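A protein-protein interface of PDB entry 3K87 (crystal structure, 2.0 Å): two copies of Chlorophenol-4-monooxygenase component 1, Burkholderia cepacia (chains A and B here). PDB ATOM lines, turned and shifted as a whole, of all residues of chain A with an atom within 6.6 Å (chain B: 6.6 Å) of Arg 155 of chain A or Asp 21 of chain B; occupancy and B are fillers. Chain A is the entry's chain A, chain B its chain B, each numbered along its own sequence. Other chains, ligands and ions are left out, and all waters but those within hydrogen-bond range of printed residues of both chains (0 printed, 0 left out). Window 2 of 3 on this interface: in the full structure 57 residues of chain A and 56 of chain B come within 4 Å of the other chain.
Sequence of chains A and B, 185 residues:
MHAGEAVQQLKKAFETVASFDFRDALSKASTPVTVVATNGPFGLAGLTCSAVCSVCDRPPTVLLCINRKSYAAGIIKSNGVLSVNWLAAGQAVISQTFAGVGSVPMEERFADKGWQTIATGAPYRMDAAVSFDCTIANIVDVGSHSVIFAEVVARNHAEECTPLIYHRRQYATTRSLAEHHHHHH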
ATOM      1  N   ILE A 118      36.773  15.713 -26.604  1.00  0.00           N
ATOM      2  CA  ILE A 118      37.172  17.016 -26.060  1.00  0.00           C
ATOM      3  C   ILE A 118      38.045  16.808 -24.830  1.00  0.00           C
ATOM      4  O   ILE A 118      39.277  16.852 -24.916  1.00  0.00           O
ATOM      5  CB  ILE A 118      35.993  17.948 -25.709  1.00  0.00           C
ATOM      6  CG1 ILE A 118      35.172  18.235 -26.949  1.00  0.00           C
ATOM      7  CG2 ILE A 118      36.511  19.280 -25.091  1.00  0.00           C
ATOM      8  CD1 ILE A 118      33.992  19.085 -26.700  1.00  0.00           C
ATOM      9  N   VAL A 130      24.175  22.243 -28.092  1.00  0.00           N
ATOM     10  CA  VAL A 130      25.007  22.307 -26.877  1.00  0.00           C
ATOM     11  C   VAL A 130      25.626  20.945 -26.719  1.00  0.00           C
ATOM     12  O   VAL A 130      24.950  19.918 -26.907  1.00  0.00           O
ATOM     13  CB  VAL A 130      24.161  22.580 -25.601  1.00  0.00           C
ATOM     14  CG1 VAL A 130      25.049  22.607 -24.328  1.00  0.00           C
ATOM     15  CG2 VAL A 130      23.392  23.868 -25.735  1.00  0.00           C
ATOM     16  N   SER A 131      26.918  20.919 -26.421  1.00  0.00           N
ATOM     17  CA  SER A 131      27.524  19.675 -25.998  1.00  0.00           C
ATOM     18  C   SER A 131      28.291  19.889 -24.710  1.00  0.00           C
ATOM     19  O   SER A 131      29.098  20.825 -24.628  1.00  0.00           O
ATOM     20  CB  SER A 131      28.418  19.098 -27.106  1.00  0.00           C
ATOM     21  OG  SER A 131      28.837  17.805 -26.715  1.00  0.00           O
ATOM     22  N   PHE A 132      28.002  19.060 -23.694  1.00  0.00           N
ATOM     23  CA  PHE A 132      28.704  19.079 -22.426  1.00  0.00           C
ATOM     24  C   PHE A 132      29.509  17.801 -22.292  1.00  0.00           C
ATOM     25  O   PHE A 132      28.943  16.717 -22.421  1.00  0.00           O
ATOM     26  CB  PHE A 132      27.724  19.080 -21.260  1.00  0.00           C
ATOM     27  CG  PHE A 132      27.116  20.421 -20.950  1.00  0.00           C
ATOM     28  CD1 PHE A 132      27.743  21.595 -21.324  1.00  0.00           C
ATOM     29  CD2 PHE A 132      25.947  20.495 -20.204  1.00  0.00           C
ATOM     30  CE1 PHE A 132      27.198  22.828 -20.964  1.00  0.00           C
ATOM     31  CE2 PHE A 132      25.383  21.729 -19.835  1.00  0.00           C
ATOM     32  CZ  PHE A 132      26.020  22.896 -20.227  1.00  0.00           C
ATOM     33  N   ASP A 133      30.810  17.917 -22.028  1.00  0.00           N
ATOM     34  CA  ASP A 133      31.664  16.753 -21.726  1.00  0.00           C
ATOM     35  C   ASP A 133      31.672  16.646 -20.214  1.00  0.00           C
ATOM     36  O   ASP A 133      31.827  17.657 -19.564  1.00  0.00           O
ATOM     37  CB  ASP A 133      33.104  16.932 -22.326  1.00  0.00           C
ATOM     38  CG  ASP A 133      33.929  15.609 -22.443  1.00  0.00           C
ATOM     39  OD1 ASP A 133      33.442  14.494 -22.105  1.00  0.00           O
ATOM     40  OD2 ASP A 133      35.109  15.675 -22.897  1.00  0.00           O
ATOM     41  N   VAL A 152      30.205  19.102 -15.384  1.00  0.00           N
ATOM     42  CA  VAL A 152      30.584  19.493 -16.729  1.00  0.00           C
ATOM     43  C   VAL A 152      32.017  19.943 -16.745  1.00  0.00           C
ATOM     44  O   VAL A 152      32.392  20.880 -16.030  1.00  0.00           O
ATOM     45  CB  VAL A 152      29.673  20.578 -17.261  1.00  0.00           C
ATOM     46  CG1 VAL A 152      30.113  20.982 -18.679  1.00  0.00           C
ATOM     47  CG2 VAL A 152      28.225  20.046 -17.298  1.00  0.00           C
ATOM     48  N   VAL A 153      32.847  19.227 -17.509  1.00  0.00           N
ATOM     49  CA  VAL A 153      34.269  19.594 -17.612  1.00  0.00           C
ATOM     50  C   VAL A 153      34.656  20.199 -18.958  1.00  0.00           C
ATOM     51  O   VAL A 153      35.753  20.722 -19.097  1.00  0.00           O
ATOM     52  CB  VAL A 153      35.214  18.409 -17.264  1.00  0.00           C
ATOM     53  CG1 VAL A 153      34.922  17.937 -15.838  1.00  0.00           C
ATOM     54  CG2 VAL A 153      35.025  17.280 -18.275  1.00  0.00           C
ATOM     55  N   ALA A 154      33.766  20.130 -19.943  1.00  0.00           N
ATOM     56  CA  ALA A 154      33.962  20.910 -21.183  1.00  0.00           C
ATOM     57  C   ALA A 154      32.627  21.230 -21.831  1.00  0.00           C
ATOM     58  O   ALA A 154      31.669  20.528 -21.579  1.00  0.00           O
ATOM     59  CB  ALA A 154      34.860  20.155 -22.148  1.00  0.00           C
ATOM     60  N   ARG A 155      32.547  22.293 -22.641  1.00  0.00           N
ATOM     61  CA  ARG A 155      31.312  22.638 -23.352  1.00  0.00           C
ATOM     62  C   ARG A 155      31.664  22.924 -24.819  1.00  0.00           C
ATOM     63  O   ARG A 155      32.797  23.276 -25.134  1.00  0.00           O
ATOM     64  CB  ARG A 155      30.635  23.888 -22.747  1.00  0.00           C
ATOM     65  CG  ARG A 155      31.459  25.130 -23.103  1.00  0.00           C
ATOM     66  CD  ARG A 155      31.082  26.444 -22.475  1.00  0.00           C
ATOM     67  NE  ARG A 155      29.997  27.091 -23.171  1.00  0.00           N
ATOM     68  CZ  ARG A 155      29.771  28.402 -23.300  1.00  0.00           C
ATOM     69  NH1 ARG A 155      30.584  29.361 -22.854  1.00  0.00           N
ATOM     70  NH2 ARG A 155      28.672  28.754 -23.935  1.00  0.00           N
ATOM     71  N   ASN A 156      30.695  22.771 -25.717  1.00  0.00           N
ATOM     72  CA  ASN A 156      30.871  23.140 -27.126  1.00  0.00           C
ATOM     73  C   ASN A 156      29.521  23.542 -27.686  1.00  0.00           C
ATOM     74  O   ASN A 156      28.488  23.115 -27.178  1.00  0.00           O
ATOM     75  CB  ASN A 156      31.428  21.958 -27.948  1.00  0.00           C
ATOM     76  CG  ASN A 156      31.881  22.377 -29.342  1.00  0.00           C
ATOM     77  OD1 ASN A 156      32.961  22.945 -29.505  1.00  0.00           O
ATOM     78  ND2 ASN A 156      31.052  22.102 -30.351  1.00  0.00           N
ATOM     79  N   HIS A 157      29.532  24.344 -28.747  1.00  0.00           N
ATOM     80  CA  HIS A 157      28.301  24.780 -29.395  1.00  0.00           C
ATOM     81  C   HIS A 157      28.472  24.836 -30.894  1.00  0.00           C
ATOM     82  O   HIS A 157      29.523  25.261 -31.377  1.00  0.00           O
ATOM     83  CB  HIS A 157      27.914  26.177 -28.939  1.00  0.00           C
ATOM     84  CG  HIS A 157      27.439  26.227 -27.534  1.00  0.00           C
ATOM     85  ND1 HIS A 157      28.214  26.719 -26.501  1.00  0.00           N
ATOM     86  CD2 HIS A 157      26.288  25.792 -26.970  1.00  0.00           C
ATOM     87  CE1 HIS A 157      27.542  26.623 -25.371  1.00  0.00           C
ATOM     88  NE2 HIS A 157      26.366  26.069 -25.630  1.00  0.00           N
ATOM     89  N   VAL B  17      34.007  23.178 -15.749  1.00  0.00           N
ATOM     90  CA  VAL B  17      33.886  24.485 -16.421  1.00  0.00           C
ATOM     91  C   VAL B  17      33.521  25.610 -15.440  1.00  0.00           C
ATOM     92  O   VAL B  17      32.944  25.358 -14.383  1.00  0.00           O
ATOM     93  CB  VAL B  17      32.837  24.473 -17.574  1.00  0.00           C
ATOM     94  CG1 VAL B  17      33.272  23.491 -18.692  1.00  0.00           C
ATOM     95  CG2 VAL B  17      31.387  24.148 -17.031  1.00  0.00           C
ATOM     96  N   ALA B  18      33.867  26.851 -15.788  1.00  0.00           N
ATOM     97  CA  ALA B  18      33.455  27.984 -14.987  1.00  0.00           C
ATOM     98  C   ALA B  18      31.916  28.058 -14.934  1.00  0.00           C
ATOM     99  O   ALA B  18      31.209  27.799 -15.934  1.00  0.00           O
ATOM    100  CB  ALA B  18      34.055  29.268 -15.563  1.00  0.00           C
ATOM    101  N   SER B  19      31.387  28.430 -13.773  1.00  0.00           N
ATOM    102  CA  SER B  19      29.955  28.578 -13.617  1.00  0.00           C
ATOM    103  C   SER B  19      29.373  29.431 -14.740  1.00  0.00           C
ATOM    104  O   SER B  19      28.280  29.144 -15.262  1.00  0.00           O
ATOM    105  CB  SER B  19      29.628  29.217 -12.275  1.00  0.00           C
ATOM    106  OG  SER B  19      30.056  28.353 -11.226  1.00  0.00           O
ATOM    107  N   PHE B  20      30.076  30.505 -15.086  1.00  0.00           N
ATOM    108  CA  PHE B  20      29.587  31.419 -16.109  1.00  0.00           C
ATOM    109  C   PHE B  20      29.430  30.735 -17.464  1.00  0.00           C
ATOM    110  O   PHE B  20      28.473  30.979 -18.180  1.00  0.00           O
ATOM    111  CB  PHE B  20      30.519  32.637 -16.272  1.00  0.00           C
ATOM    112  CG  PHE B  20      30.098  33.507 -17.389  1.00  0.00           C
ATOM    113  CD1 PHE B  20      29.323  34.633 -17.151  1.00  0.00           C
ATOM    114  CD2 PHE B  20      30.408  33.155 -18.692  1.00  0.00           C
ATOM    115  CE1 PHE B  20      28.871  35.416 -18.202  1.00  0.00           C
ATOM    116  CE2 PHE B  20      29.943  33.927 -19.778  1.00  0.00           C
ATOM    117  CZ  PHE B  20      29.183  35.070 -19.519  1.00  0.00           C
ATOM    118  N   ASP B  21      30.397  29.888 -17.817  1.00  0.00           N
ATOM    119  CA  ASP B  21      30.321  29.086 -19.050  1.00  0.00           C
ATOM    120  C   ASP B  21      29.138  28.116 -19.050  1.00  0.00           C
ATOM    121  O   ASP B  21      28.433  27.945 -20.055  1.00  0.00           O
ATOM    122  CB  ASP B  21      31.632  28.331 -19.244  1.00  0.00           C
ATOM    123  CG  ASP B  21      32.729  29.241 -19.779  1.00  0.00           C
ATOM    124  OD1 ASP B  21      32.425  30.014 -20.716  1.00  0.00           O
ATOM    125  OD2 ASP B  21      33.852  29.205 -19.252  1.00  0.00           O
ATOM    126  N   PHE B  22      28.948  27.458 -17.922  1.00  0.00           N
ATOM    127  CA  PHE B  22      27.809  26.537 -17.749  1.00  0.00           C
ATOM    128  C   PHE B  22      26.485  27.251 -18.047  1.00  0.00           C
ATOM    129  O   PHE B  22      25.685  26.745 -18.824  1.00  0.00           O
ATOM    130  CB  PHE B  22      27.817  26.002 -16.326  1.00  0.00           C
ATOM    131  CG  PHE B  22      26.679  25.027 -15.995  1.00  0.00           C
ATOM    132  CD1 PHE B  22      25.636  25.417 -15.169  1.00  0.00           C
ATOM    133  CD2 PHE B  22      26.698  23.726 -16.490  1.00  0.00           C
ATOM    134  CE1 PHE B  22      24.614  24.533 -14.846  1.00  0.00           C
ATOM    135  CE2 PHE B  22      25.702  22.822 -16.165  1.00  0.00           C
ATOM    136  CZ  PHE B  22      24.665  23.208 -15.336  1.00  0.00           C
ATOM    137  N   ARG B  23      26.260  28.405 -17.403  1.00  0.00           N
ATOM    138  CA  ARG B  23      25.001  29.166 -17.537  1.00  0.00           C
ATOM    139  C   ARG B  23      24.819  29.632 -18.981  1.00  0.00           C
ATOM    140  O   ARG B  23      23.747  29.518 -19.566  1.00  0.00           O
ATOM    141  CB  ARG B  23      24.980  30.380 -16.588  1.00  0.00           C
ATOM    142  CG  ARG B  23      25.048  30.019 -15.126  1.00  0.00           C
ATOM    143  CD  ARG B  23      24.704  31.201 -14.221  1.00  0.00           C
ATOM    144  NE  ARG B  23      25.530  32.394 -14.412  1.00  0.00           N
ATOM    145  CZ  ARG B  23      26.654  32.693 -13.747  1.00  0.00           C
ATOM    146  NH1 ARG B  23      27.176  31.844 -12.851  1.00  0.00           N
ATOM    147  NH2 ARG B  23      27.274  33.846 -13.997  1.00  0.00           N
ATOM    148  N   ASP B  24      25.894  30.118 -19.572  1.00  0.00           N
ATOM    149  CA  ASP B  24      25.828  30.582 -20.954  1.00  0.00           C
ATOM    150  C   ASP B  24      25.421  29.437 -21.855  1.00  0.00           C
ATOM    151  O   ASP B  24      24.507  29.557 -22.679  1.00  0.00           O
ATOM    152  CB  ASP B  24      27.204  31.105 -21.400  1.00  0.00           C
ATOM    153  CG  ASP B  24      27.185  31.557 -22.831  1.00  0.00           C
ATOM    154  OD1 ASP B  24      28.232  31.501 -23.485  1.00  0.00           O
ATOM    155  OD2 ASP B  24      26.114  31.973 -23.295  1.00  0.00           O
ATOM    156  N   ALA B  25      26.094  28.309 -21.684  1.00  0.00           N
ATOM    157  CA  ALA B  25      25.774  27.137 -22.497  1.00  0.00           C
ATOM    158  C   ALA B  25      24.314  26.767 -22.360  1.00  0.00           C
ATOM    159  O   ALA B  25      23.654  26.506 -23.369  1.00  0.00           O
ATOM    160  CB  ALA B  25      26.642  25.988 -22.135  1.00  0.00           C
ATOM    161  N   LEU B  26      23.802  26.743 -21.124  1.00  0.00           N
ATOM    162  CA  LEU B  26      22.416  26.352 -20.902  1.00  0.00           C
ATOM    163  C   LEU B  26      21.433  27.258 -21.634  1.00  0.00           C
ATOM    164  O   LEU B  26      20.374  26.770 -22.038  1.00  0.00           O
ATOM    165  CB  LEU B  26      22.051  26.366 -19.418  1.00  0.00           C
ATOM    166  CG  LEU B  26      22.682  25.214 -18.617  1.00  0.00           C
ATOM    167  CD1 LEU B  26      22.233  25.330 -17.172  1.00  0.00           C
ATOM    168  CD2 LEU B  26      22.335  23.866 -19.225  1.00  0.00           C
ATOM    169  N   LYS B  28      21.568  28.243 -24.444  1.00  0.00           N
ATOM    170  CA  LYS B  28      21.549  27.781 -25.809  1.00  0.00           C
ATOM    171  C   LYS B  28      20.814  26.443 -25.932  1.00  0.00           C
ATOM    172  O   LYS B  28      20.504  26.004 -27.048  1.00  0.00           O
ATOM    173  CB  LYS B  28      22.982  27.697 -26.357  1.00  0.00           C
ATOM    174  CG  LYS B  28      23.663  29.080 -26.573  1.00  0.00           C
ATOM    175  CD  LYS B  28      25.159  28.918 -26.990  1.00  0.00           C
ATOM    176  CE  LYS B  28      25.657  29.985 -27.989  1.00  0.00           C
ATOM    177  NZ  LYS B  28      25.301  29.616 -29.425  1.00  0.00           N
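NH2 of Arg 155 of chain A is in salt-bridge range of OD1 of Asp 24 of chain B. The backbone carbonyl oxygen (O) of Val 152 of chain A sits at hydrogen-bond distance from the backbone NH (N) of Val 17 of chain B (2.8 Å). NH1 of Arg 155 of chain A lies within salt-bridge range of OD1 of Asp 21 of chain B. The guanidinium group of Arg 155 of chain A lies close to the backbone NH of Ala 25 of chain B (3.5 Å).
A ring nitrogen (ND1) of His 157 of chain A sits close to the guanidinium group of Arg 155 of chain A. O of Asp 133 of chain A sits at hydrogen-bond distance from N of Val 153 of chain A (2.8 Å). The backbone carbonyl oxygen (O) of Ala 154 of chain A lies within hydrogen-bond range of the backbone NH (N) of Asp 133 of chain A, 2.8 Å away.
No position is printed for both chains. Of the 14 pairs that touch across the chains among the printed residues, none has its exchanged pair printed and touching as well.
Of the printed residues of chain B, Val 130 of chain A touches Ala 25 and Lys 28. Asp 133 of chain A touches none of the printed residues of chain B. Of the printed residues of chain B, Val 153 of chain A touches Val 17 (3.6 Å). Printed residues of chain B within 4 Å of Ala 154 of chain A: Val 17 (3.6 Å). Arg 155 of chain A touches three residues of chain B. Ser 19 of chain B touches none of the printed residues of chain A. Printed residues of chain A within 4 Å of Phe 22 of chain B: Phe 132 (3.8 Å) and Val 152 (3.9 Å). Of the printed residues of chain A, Asp 24 of chain B touches Arg 155 (2.8 Å). The nearest residue of chain B that does not touch Arg 155 of chain A is Val 17 of chain B (4.2 Å).
CG2 of Val 130 of chain A touches O of Ala 25 of chain B, at 3.6 Å. C of Lys 28 of chain B touches CG2 of Val 130 of chain A, 3.6 Å away. Phe 132 of chain A touches Phe 22 of chain B. Phe 132 of chain A touches Ala 25 of chain B (CE1 to CB, 3.4 Å). CE2 of Phe 132 of chain A touches CD2 of Leu 26 of chain B, 3.8 Å away. Val 152 of chain A touches Phe 22 of chain B. CG1 of Val 17 of chain B touches C of Val 153 of chain A, 3.6 Å away. Val 17 of chain B touches Ala 154 of chain A (CG1 to N, 3.6 Å). Ala 25 of chain B touches His 157 of chain A. His 157 of chain A touches Lys 28 of chain B.
Hydrophobic or aromatic side chains of chain A that line the printed part of chain B: Val 130, Phe 132, Val 152 and His 157. Along chain A the printed residues that touch a printed residue of chain B span positions 130 to 157. Hydrophobic or aromatic side chains of chain B that line the printed part of chain A: Val 17, Phe 22, Ala 25 and Leu 26. Among the printed residues, 14 pairs touch across the chains. Among the printed residues, Asp or Glu carboxylates within 4 Å of a Lys or Arg side-chain nitrogen of the other chain: Arg 155 of chain A with Asp 21 of chain B (2.9 Å) and Arg 155 of chain A with Asp 24 of chain B (2.8 Å).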
